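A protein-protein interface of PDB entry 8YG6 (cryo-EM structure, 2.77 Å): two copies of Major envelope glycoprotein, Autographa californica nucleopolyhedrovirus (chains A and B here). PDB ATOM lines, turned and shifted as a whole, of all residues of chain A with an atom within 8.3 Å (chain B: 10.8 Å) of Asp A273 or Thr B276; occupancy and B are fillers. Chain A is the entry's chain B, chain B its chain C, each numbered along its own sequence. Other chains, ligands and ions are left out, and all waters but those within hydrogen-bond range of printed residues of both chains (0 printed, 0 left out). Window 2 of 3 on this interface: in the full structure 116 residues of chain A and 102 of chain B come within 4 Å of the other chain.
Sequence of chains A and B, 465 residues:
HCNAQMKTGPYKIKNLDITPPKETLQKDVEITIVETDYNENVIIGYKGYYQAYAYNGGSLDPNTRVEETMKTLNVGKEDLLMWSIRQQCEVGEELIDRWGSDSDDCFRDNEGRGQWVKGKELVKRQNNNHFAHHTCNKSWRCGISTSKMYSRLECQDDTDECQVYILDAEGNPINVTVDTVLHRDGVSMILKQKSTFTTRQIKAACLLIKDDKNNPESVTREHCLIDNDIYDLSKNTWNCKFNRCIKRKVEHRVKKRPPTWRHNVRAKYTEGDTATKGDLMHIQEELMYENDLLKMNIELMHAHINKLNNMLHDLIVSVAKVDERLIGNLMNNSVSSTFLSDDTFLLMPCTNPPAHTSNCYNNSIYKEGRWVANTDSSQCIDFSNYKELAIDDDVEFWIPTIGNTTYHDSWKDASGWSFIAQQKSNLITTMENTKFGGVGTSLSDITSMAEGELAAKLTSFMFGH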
ATOM      1  N   TRP A 261     -25.626  24.096  -3.890  1.00  0.00           N
ATOM      2  CA  TRP A 261     -24.485  23.399  -4.461  1.00  0.00           C
ATOM      3  C   TRP A 261     -23.827  24.244  -5.544  1.00  0.00           C
ATOM      4  O   TRP A 261     -24.496  24.739  -6.455  1.00  0.00           O
ATOM      5  CB  TRP A 261     -24.919  22.052  -5.040  1.00  0.00           C
ATOM      6  CG  TRP A 261     -23.796  21.252  -5.622  1.00  0.00           C
ATOM      7  CD1 TRP A 261     -23.025  20.332  -4.974  1.00  0.00           C
ATOM      8  CD2 TRP A 261     -23.321  21.292  -6.973  1.00  0.00           C
ATOM      9  NE1 TRP A 261     -22.097  19.801  -5.836  1.00  0.00           N
ATOM     10  CE2 TRP A 261     -22.257  20.374  -7.070  1.00  0.00           C
ATOM     11  CE3 TRP A 261     -23.692  22.017  -8.110  1.00  0.00           C
ATOM     12  CZ2 TRP A 261     -21.561  20.160  -8.258  1.00  0.00           C
ATOM     13  CZ3 TRP A 261     -22.998  21.805  -9.289  1.00  0.00           C
ATOM     14  CH2 TRP A 261     -21.946  20.884  -9.353  1.00  0.00           C
ATOM     15  N   ALA A 267     -18.847  19.362  -1.600  1.00  0.00           N
ATOM     16  CA  ALA A 267     -20.282  19.088  -1.568  1.00  0.00           C
ATOM     17  C   ALA A 267     -20.571  18.050  -0.487  1.00  0.00           C
ATOM     18  O   ALA A 267     -20.660  16.855  -0.775  1.00  0.00           O
ATOM     19  CB  ALA A 267     -20.773  18.620  -2.932  1.00  0.00           C
ATOM     20  N   TYR A 269     -20.933  15.275   2.110  1.00  0.00           N
ATOM     21  CA  TYR A 269     -20.220  14.007   2.179  1.00  0.00           C
ATOM     22  C   TYR A 269     -19.555  13.693   0.846  1.00  0.00           C
ATOM     23  O   TYR A 269     -20.068  14.035  -0.223  1.00  0.00           O
ATOM     24  CB  TYR A 269     -21.177  12.881   2.570  1.00  0.00           C
ATOM     25  CG  TYR A 269     -22.544  12.986   1.931  1.00  0.00           C
ATOM     26  CD1 TYR A 269     -22.776  12.486   0.656  1.00  0.00           C
ATOM     27  CD2 TYR A 269     -23.601  13.587   2.600  1.00  0.00           C
ATOM     28  CE1 TYR A 269     -24.022  12.579   0.068  1.00  0.00           C
ATOM     29  CE2 TYR A 269     -24.851  13.684   2.022  1.00  0.00           C
ATOM     30  CZ  TYR A 269     -25.057  13.180   0.757  1.00  0.00           C
ATOM     31  OH  TYR A 269     -26.300  13.279   0.178  1.00  0.00           O
ATOM     32  N   THR A 270     -18.403  13.032   0.914  1.00  0.00           N
ATOM     33  CA  THR A 270     -17.599  12.710  -0.257  1.00  0.00           C
ATOM     34  C   THR A 270     -17.823  11.255  -0.637  1.00  0.00           C
ATOM     35  O   THR A 270     -17.639  10.358   0.193  1.00  0.00           O
ATOM     36  CB  THR A 270     -16.115  12.969   0.008  1.00  0.00           C
ATOM     37  OG1 THR A 270     -15.919  14.356   0.309  1.00  0.00           O
ATOM     38  CG2 THR A 270     -15.286  12.604  -1.211  1.00  0.00           C
ATOM     39  N   GLU A 271     -18.214  11.025  -1.887  1.00  0.00           N
ATOM     40  CA  GLU A 271     -18.378   9.686  -2.444  1.00  0.00           C
ATOM     41  C   GLU A 271     -17.612   9.640  -3.758  1.00  0.00           C
ATOM     42  O   GLU A 271     -18.117  10.095  -4.792  1.00  0.00           O
ATOM     43  CB  GLU A 271     -19.854   9.350  -2.654  1.00  0.00           C
ATOM     44  CG  GLU A 271     -20.574   8.883  -1.399  1.00  0.00           C
ATOM     45  CD  GLU A 271     -21.931   8.276  -1.693  1.00  0.00           C
ATOM     46  OE1 GLU A 271     -22.399   8.387  -2.846  1.00  0.00           O
ATOM     47  OE2 GLU A 271     -22.531   7.687  -0.770  1.00  0.00           O
ATOM     48  N   GLY A 272     -16.399   9.094  -3.722  1.00  0.00           N
ATOM     49  CA  GLY A 272     -15.551   9.114  -4.897  1.00  0.00           C
ATOM     50  C   GLY A 272     -15.913   8.068  -5.931  1.00  0.00           C
ATOM     51  O   GLY A 272     -15.599   6.886  -5.769  1.00  0.00           O
ATOM     52  N   ASP A 273     -16.545   8.512  -7.011  1.00  0.00           N
ATOM     53  CA  ASP A 273     -16.960   7.675  -8.134  1.00  0.00           C
ATOM     54  C   ASP A 273     -17.025   8.571  -9.365  1.00  0.00           C
ATOM     55  O   ASP A 273     -16.644   9.744  -9.324  1.00  0.00           O
ATOM     56  CB  ASP A 273     -18.305   6.990  -7.881  1.00  0.00           C
ATOM     57  CG  ASP A 273     -18.205   5.813  -6.931  1.00  0.00           C
ATOM     58  OD1 ASP A 273     -17.165   5.121  -6.943  1.00  0.00           O
ATOM     59  OD2 ASP A 273     -19.167   5.577  -6.172  1.00  0.00           O
ATOM     60  N   THR A 274     -17.511   8.005 -10.465  1.00  0.00           N
ATOM     61  CA  THR A 274     -17.703   8.741 -11.708  1.00  0.00           C
ATOM     62  C   THR A 274     -19.164   8.649 -12.121  1.00  0.00           C
ATOM     63  O   THR A 274     -19.707   7.548 -12.253  1.00  0.00           O
ATOM     64  CB  THR A 274     -16.803   8.196 -12.818  1.00  0.00           C
ATOM     65  OG1 THR A 274     -15.430   8.304 -12.416  1.00  0.00           O
ATOM     66  CG2 THR A 274     -17.010   8.979 -14.103  1.00  0.00           C
ATOM     67  N   ALA A 275     -19.794   9.803 -12.322  1.00  0.00           N
ATOM     68  CA  ALA A 275     -21.185   9.838 -12.738  1.00  0.00           C
ATOM     69  C   ALA A 275     -21.306   9.579 -14.238  1.00  0.00           C
ATOM     70  O   ALA A 275     -20.356   9.752 -15.006  1.00  0.00           O
ATOM     71  CB  ALA A 275     -21.821  11.181 -12.384  1.00  0.00           C
ATOM     72  N   THR A 276     -22.498   9.156 -14.647  1.00  0.00           N
ATOM     73  CA  THR A 276     -22.798   8.862 -16.039  1.00  0.00           C
ATOM     74  C   THR A 276     -24.085   9.568 -16.440  1.00  0.00           C
ATOM     75  O   THR A 276     -24.837  10.069 -15.598  1.00  0.00           O
ATOM     76  CB  THR A 276     -22.918   7.352 -16.287  1.00  0.00           C
ATOM     77  OG1 THR A 276     -23.922   6.802 -15.425  1.00  0.00           O
ATOM     78  CG2 THR A 276     -21.590   6.658 -16.023  1.00  0.00           C
ATOM     79  N   ASP A 279     -27.645   8.348 -14.923  1.00  0.00           N
ATOM     80  CA  ASP A 279     -28.064   8.838 -13.614  1.00  0.00           C
ATOM     81  C   ASP A 279     -28.698  10.219 -13.722  1.00  0.00           C
ATOM     82  O   ASP A 279     -29.735  10.489 -13.099  1.00  0.00           O
ATOM     83  CB  ASP A 279     -26.868   8.875 -12.663  1.00  0.00           C
ATOM     84  CG  ASP A 279     -26.182   7.530 -12.537  1.00  0.00           C
ATOM     85  OD1 ASP A 279     -26.859   6.495 -12.708  1.00  0.00           O
ATOM     86  OD2 ASP A 279     -24.963   7.508 -12.267  1.00  0.00           O
ATOM     87  N   ASP B 273     -14.386  18.855 -15.829  1.00  0.00           N
ATOM     88  CA  ASP B 273     -14.120  18.207 -14.548  1.00  0.00           C
ATOM     89  C   ASP B 273     -14.829  16.859 -14.566  1.00  0.00           C
ATOM     90  O   ASP B 273     -15.385  16.444 -15.588  1.00  0.00           O
ATOM     91  CB  ASP B 273     -14.585  19.056 -13.361  1.00  0.00           C
ATOM     92  CG  ASP B 273     -13.658  20.219 -13.061  1.00  0.00           C
ATOM     93  OD1 ASP B 273     -12.434  20.076 -13.262  1.00  0.00           O
ATOM     94  OD2 ASP B 273     -14.154  21.277 -12.623  1.00  0.00           O
ATOM     95  N   THR B 274     -14.805  16.177 -13.426  1.00  0.00           N
ATOM     96  CA  THR B 274     -15.492  14.905 -13.257  1.00  0.00           C
ATOM     97  C   THR B 274     -16.474  15.018 -12.101  1.00  0.00           C
ATOM     98  O   THR B 274     -16.087  15.384 -10.986  1.00  0.00           O
ATOM     99  CB  THR B 274     -14.498  13.770 -12.998  1.00  0.00           C
ATOM    100  OG1 THR B 274     -13.591  13.669 -14.103  1.00  0.00           O
ATOM    101  CG2 THR B 274     -15.232  12.449 -12.832  1.00  0.00           C
ATOM    102  N   ALA B 275     -17.739  14.708 -12.368  1.00  0.00           N
ATOM    103  CA  ALA B 275     -18.762  14.761 -11.337  1.00  0.00           C
ATOM    104  C   ALA B 275     -18.704  13.515 -10.458  1.00  0.00           C
ATOM    105  O   ALA B 275     -18.173  12.471 -10.843  1.00  0.00           O
ATOM    106  CB  ALA B 275     -20.150  14.902 -11.961  1.00  0.00           C
ATOM    107  N   THR B 276     -19.262  13.642  -9.257  1.00  0.00           N
ATOM    108  CA  THR B 276     -19.305  12.560  -8.287  1.00  0.00           C
ATOM    109  C   THR B 276     -20.727  12.403  -7.764  1.00  0.00           C
ATOM    110  O   THR B 276     -21.590  13.260  -7.974  1.00  0.00           O
ATOM    111  CB  THR B 276     -18.333  12.803  -7.124  1.00  0.00           C
ATOM    112  OG1 THR B 276     -18.635  14.056  -6.500  1.00  0.00           O
ATOM    113  CG2 THR B 276     -16.896  12.819  -7.621  1.00  0.00           C
ATOM    114  N   LYS B 277     -20.961  11.285  -7.076  1.00  0.00           N
ATOM    115  CA  LYS B 277     -22.302  10.974  -6.585  1.00  0.00           C
ATOM    116  C   LYS B 277     -22.767  11.985  -5.543  1.00  0.00           C
ATOM    117  O   LYS B 277     -23.968  12.269  -5.436  1.00  0.00           O
ATOM    118  CB  LYS B 277     -22.323   9.559  -6.006  1.00  0.00           C
ATOM    119  CG  LYS B 277     -21.697   8.509  -6.912  1.00  0.00           C
ATOM    120  CD  LYS B 277     -22.669   8.030  -7.978  1.00  0.00           C
ATOM    121  CE  LYS B 277     -22.130   6.802  -8.693  1.00  0.00           C
ATOM    122  NZ  LYS B 277     -22.965   6.431  -9.869  1.00  0.00           N
ATOM    123  N   GLY B 278     -21.830  12.529  -4.761  1.00  0.00           N
ATOM    124  CA  GLY B 278     -22.203  13.471  -3.718  1.00  0.00           C
ATOM    125  C   GLY B 278     -22.871  14.718  -4.261  1.00  0.00           C
ATOM    126  O   GLY B 278     -23.848  15.209  -3.692  1.00  0.00           O
ATOM    127  N   ASP B 279     -22.351  15.249  -5.373  1.00  0.00           N
ATOM    128  CA  ASP B 279     -22.959  16.427  -5.981  1.00  0.00           C
ATOM    129  C   ASP B 279     -24.384  16.137  -6.433  1.00  0.00           C
ATOM    130  O   ASP B 279     -25.293  16.952  -6.219  1.00  0.00           O
ATOM    131  CB  ASP B 279     -22.111  16.899  -7.163  1.00  0.00           C
ATOM    132  CG  ASP B 279     -20.674  17.179  -6.773  1.00  0.00           C
ATOM    133  OD1 ASP B 279     -20.429  17.532  -5.601  1.00  0.00           O
ATOM    134  OD2 ASP B 279     -19.786  17.043  -7.642  1.00  0.00           O
ATOM    135  N   LEU B 280     -24.597  14.976  -7.054  1.00  0.00           N
ATOM    136  CA  LEU B 280     -25.927  14.617  -7.527  1.00  0.00           C
ATOM    137  C   LEU B 280     -26.900  14.475  -6.364  1.00  0.00           C
ATOM    138  O   LEU B 280     -28.044  14.944  -6.432  1.00  0.00           O
ATOM    139  CB  LEU B 280     -25.859  13.326  -8.342  1.00  0.00           C
ATOM    140  CG  LEU B 280     -27.089  13.010  -9.191  1.00  0.00           C
ATOM    141  CD1 LEU B 280     -27.291  14.093 -10.233  1.00  0.00           C
ATOM    142  CD2 LEU B 280     -26.938  11.654  -9.856  1.00  0.00           C
ATOM    143  N   MET B 281     -26.459  13.836  -5.277  1.00  0.00           N
ATOM    144  CA  MET B 281     -27.324  13.700  -4.107  1.00  0.00           C
ATOM    145  C   MET B 281     -27.624  15.051  -3.467  1.00  0.00           C
ATOM    146  O   MET B 281     -28.747  15.279  -3.004  1.00  0.00           O
ATOM    147  CB  MET B 281     -26.691  12.744  -3.098  1.00  0.00           C
ATOM    148  CG  MET B 281     -26.607  11.310  -3.600  1.00  0.00           C
ATOM    149  SD  MET B 281     -25.922  10.159  -2.394  1.00  0.00           S
ATOM    150  CE  MET B 281     -24.190  10.605  -2.446  1.00  0.00           C
ATOM    151  N   HIS B 282     -26.640  15.955  -3.432  1.00  0.00           N
ATOM    152  CA  HIS B 282     -26.870  17.300  -2.915  1.00  0.00           C
ATOM    153  C   HIS B 282     -27.937  18.024  -3.733  1.00  0.00           C
ATOM    154  O   HIS B 282     -28.865  18.631  -3.176  1.00  0.00           O
ATOM    155  CB  HIS B 282     -25.553  18.079  -2.930  1.00  0.00           C
ATOM    156  CG  HIS B 282     -25.545  19.283  -2.040  1.00  0.00           C
ATOM    157  ND1 HIS B 282     -24.450  19.636  -1.285  1.00  0.00           N
ATOM    158  CD2 HIS B 282     -26.491  20.219  -1.796  1.00  0.00           C
ATOM    159  CE1 HIS B 282     -24.720  20.737  -0.607  1.00  0.00           C
ATOM    160  NE2 HIS B 282     -25.954  21.113  -0.898  1.00  0.00           N
ATOM    161  N   ILE B 283     -27.818  17.962  -5.062  1.00  0.00           N
ATOM    162  CA  ILE B 283     -28.805  18.598  -5.933  1.00  0.00           C
ATOM    163  C   ILE B 283     -30.184  17.993  -5.703  1.00  0.00           C
ATOM    164  O   ILE B 283     -31.192  18.712  -5.611  1.00  0.00           O
ATOM    165  CB  ILE B 283     -28.371  18.477  -7.404  1.00  0.00           C
ATOM    166  CG1 ILE B 283     -27.023  19.167  -7.627  1.00  0.00           C
ATOM    167  CG2 ILE B 283     -29.416  19.076  -8.324  1.00  0.00           C
ATOM    168  CD1 ILE B 283     -27.061  20.658  -7.402  1.00  0.00           C
ATOM    169  N   GLN B 284     -30.248  16.663  -5.598  1.00  0.00           N
ATOM    170  CA  GLN B 284     -31.522  15.987  -5.384  1.00  0.00           C
ATOM    171  C   GLN B 284     -32.172  16.439  -4.083  1.00  0.00           C
ATOM    172  O   GLN B 284     -33.374  16.726  -4.041  1.00  0.00           O
ATOM    173  CB  GLN B 284     -31.305  14.473  -5.386  1.00  0.00           C
ATOM    174  CG  GLN B 284     -32.563  13.650  -5.578  1.00  0.00           C
ATOM    175  CD  GLN B 284     -32.319  12.169  -5.362  1.00  0.00           C
ATOM    176  OE1 GLN B 284     -31.447  11.780  -4.585  1.00  0.00           O
ATOM    177  NE2 GLN B 284     -33.086  11.333  -6.050  1.00  0.00           N
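Asp A273 touches Ala B275, but with the chains exchanged Ala A275 does not touch Asp B273 (8.4 Å). Asp A273 touches Thr B276, but with the chains exchanged Thr A276 does not touch Asp B273 (10.2 Å). Thr A274 touches Ala B275, but with the chains exchanged Ala A275 does not touch Thr B274 (5.3 Å). Ala A275 touches its own counterpart, Ala B275. 5 positions are printed for both chains. Of the 15 pairs that touch across the chains among the printed residues, 1 has its exchanged pair printed and touching as well.
Of chain A, only Glu A271 (3.6 Å) and Asp A273 (3.5 Å) come within 4 Å of Thr B276. Of chain B, only Thr B276, Lys B277 and Met B281 come within 4 Å of Glu A271. No residue of chain B comes within 4 Å of Gly A272. Thr A274 touches just one residue of chain B: Ala B275 (3.9 Å). Ala A275 touches just one residue of chain B: Ala B275 (3.5 Å). Printed residues of chain A within 4 Å of Ala B275: Asp A273, Thr A274 and Ala A275. Of the printed residues of chain A, Lys B277 touches Glu A271, Asp A273 and Asp A279. Printed residues of chain A within 4 Å of Asp B279: Trp A261 and Ala A267. Of the printed residues of chain A, Leu B280 touches Asp A279. Of the printed residues of chain B, Trp A261 touches Asp B279, His B282 and Ile B283. The nearest printed residue of chain B that does not touch Ala A267 is His B282 (4.2 Å).
The backbone carbonyl oxygen (O) of Ala B275 sits at hydrogen-bond distance from the backbone NH (N) of Ala A275, 3.5 Å away. NZ of Lys B277 is in salt-bridge range of OD2 of Asp A279. The backbone carbonyl oxygen of Ala B275 sits close to the backbone carbonyl oxygen of Asp A273 (3.5 Å). NE1 of Trp A261 is in hydrogen-bond range of OD1 of Asp B279 (2.8 Å).
OD2 of Asp A279 sits at hydrogen-bond distance from OG1 of Thr A276, at 3.4 Å. OG1 of Thr B276 sits at hydrogen-bond distance from OD2 of Asp B279, at 3.4 Å.
Trp A261 touches His B282. Trp A261 touches Ile B283. Tyr A269 touches Met B281 (CE1 to CE, 3.2 Å). Thr B276 touches Glu A271. Glu A271 touches Lys B277. Met B281 touches Glu A271 (CE to OE1, 2.9 Å). Thr B276 touches Asp A273. CB of Asp A273 touches CG of Lys B277, at 3.8 Å. CA of Thr A274 touches O of Ala B275 (3.9 Å). CB of Asp A279 touches CD2 of Leu B280, 3.95 Å away.
Hydrophobic or aromatic side chains of chain B within 4 Å of the printed part of chain A: Leu B280, Met B281, His B282 and Ile B283. Hydrophobic or aromatic side chains of chain A within 4 Å of the printed part of chain B: Trp A261, Ala A267 and Tyr A269. Along chain A the printed residues that touch a printed residue of chain B span positions 261 to 279. Among the printed residues, Asp or Glu carboxylates within 4 Å of a Lys or Arg side-chain nitrogen of the other chain: Asp A279 with Lys B277.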
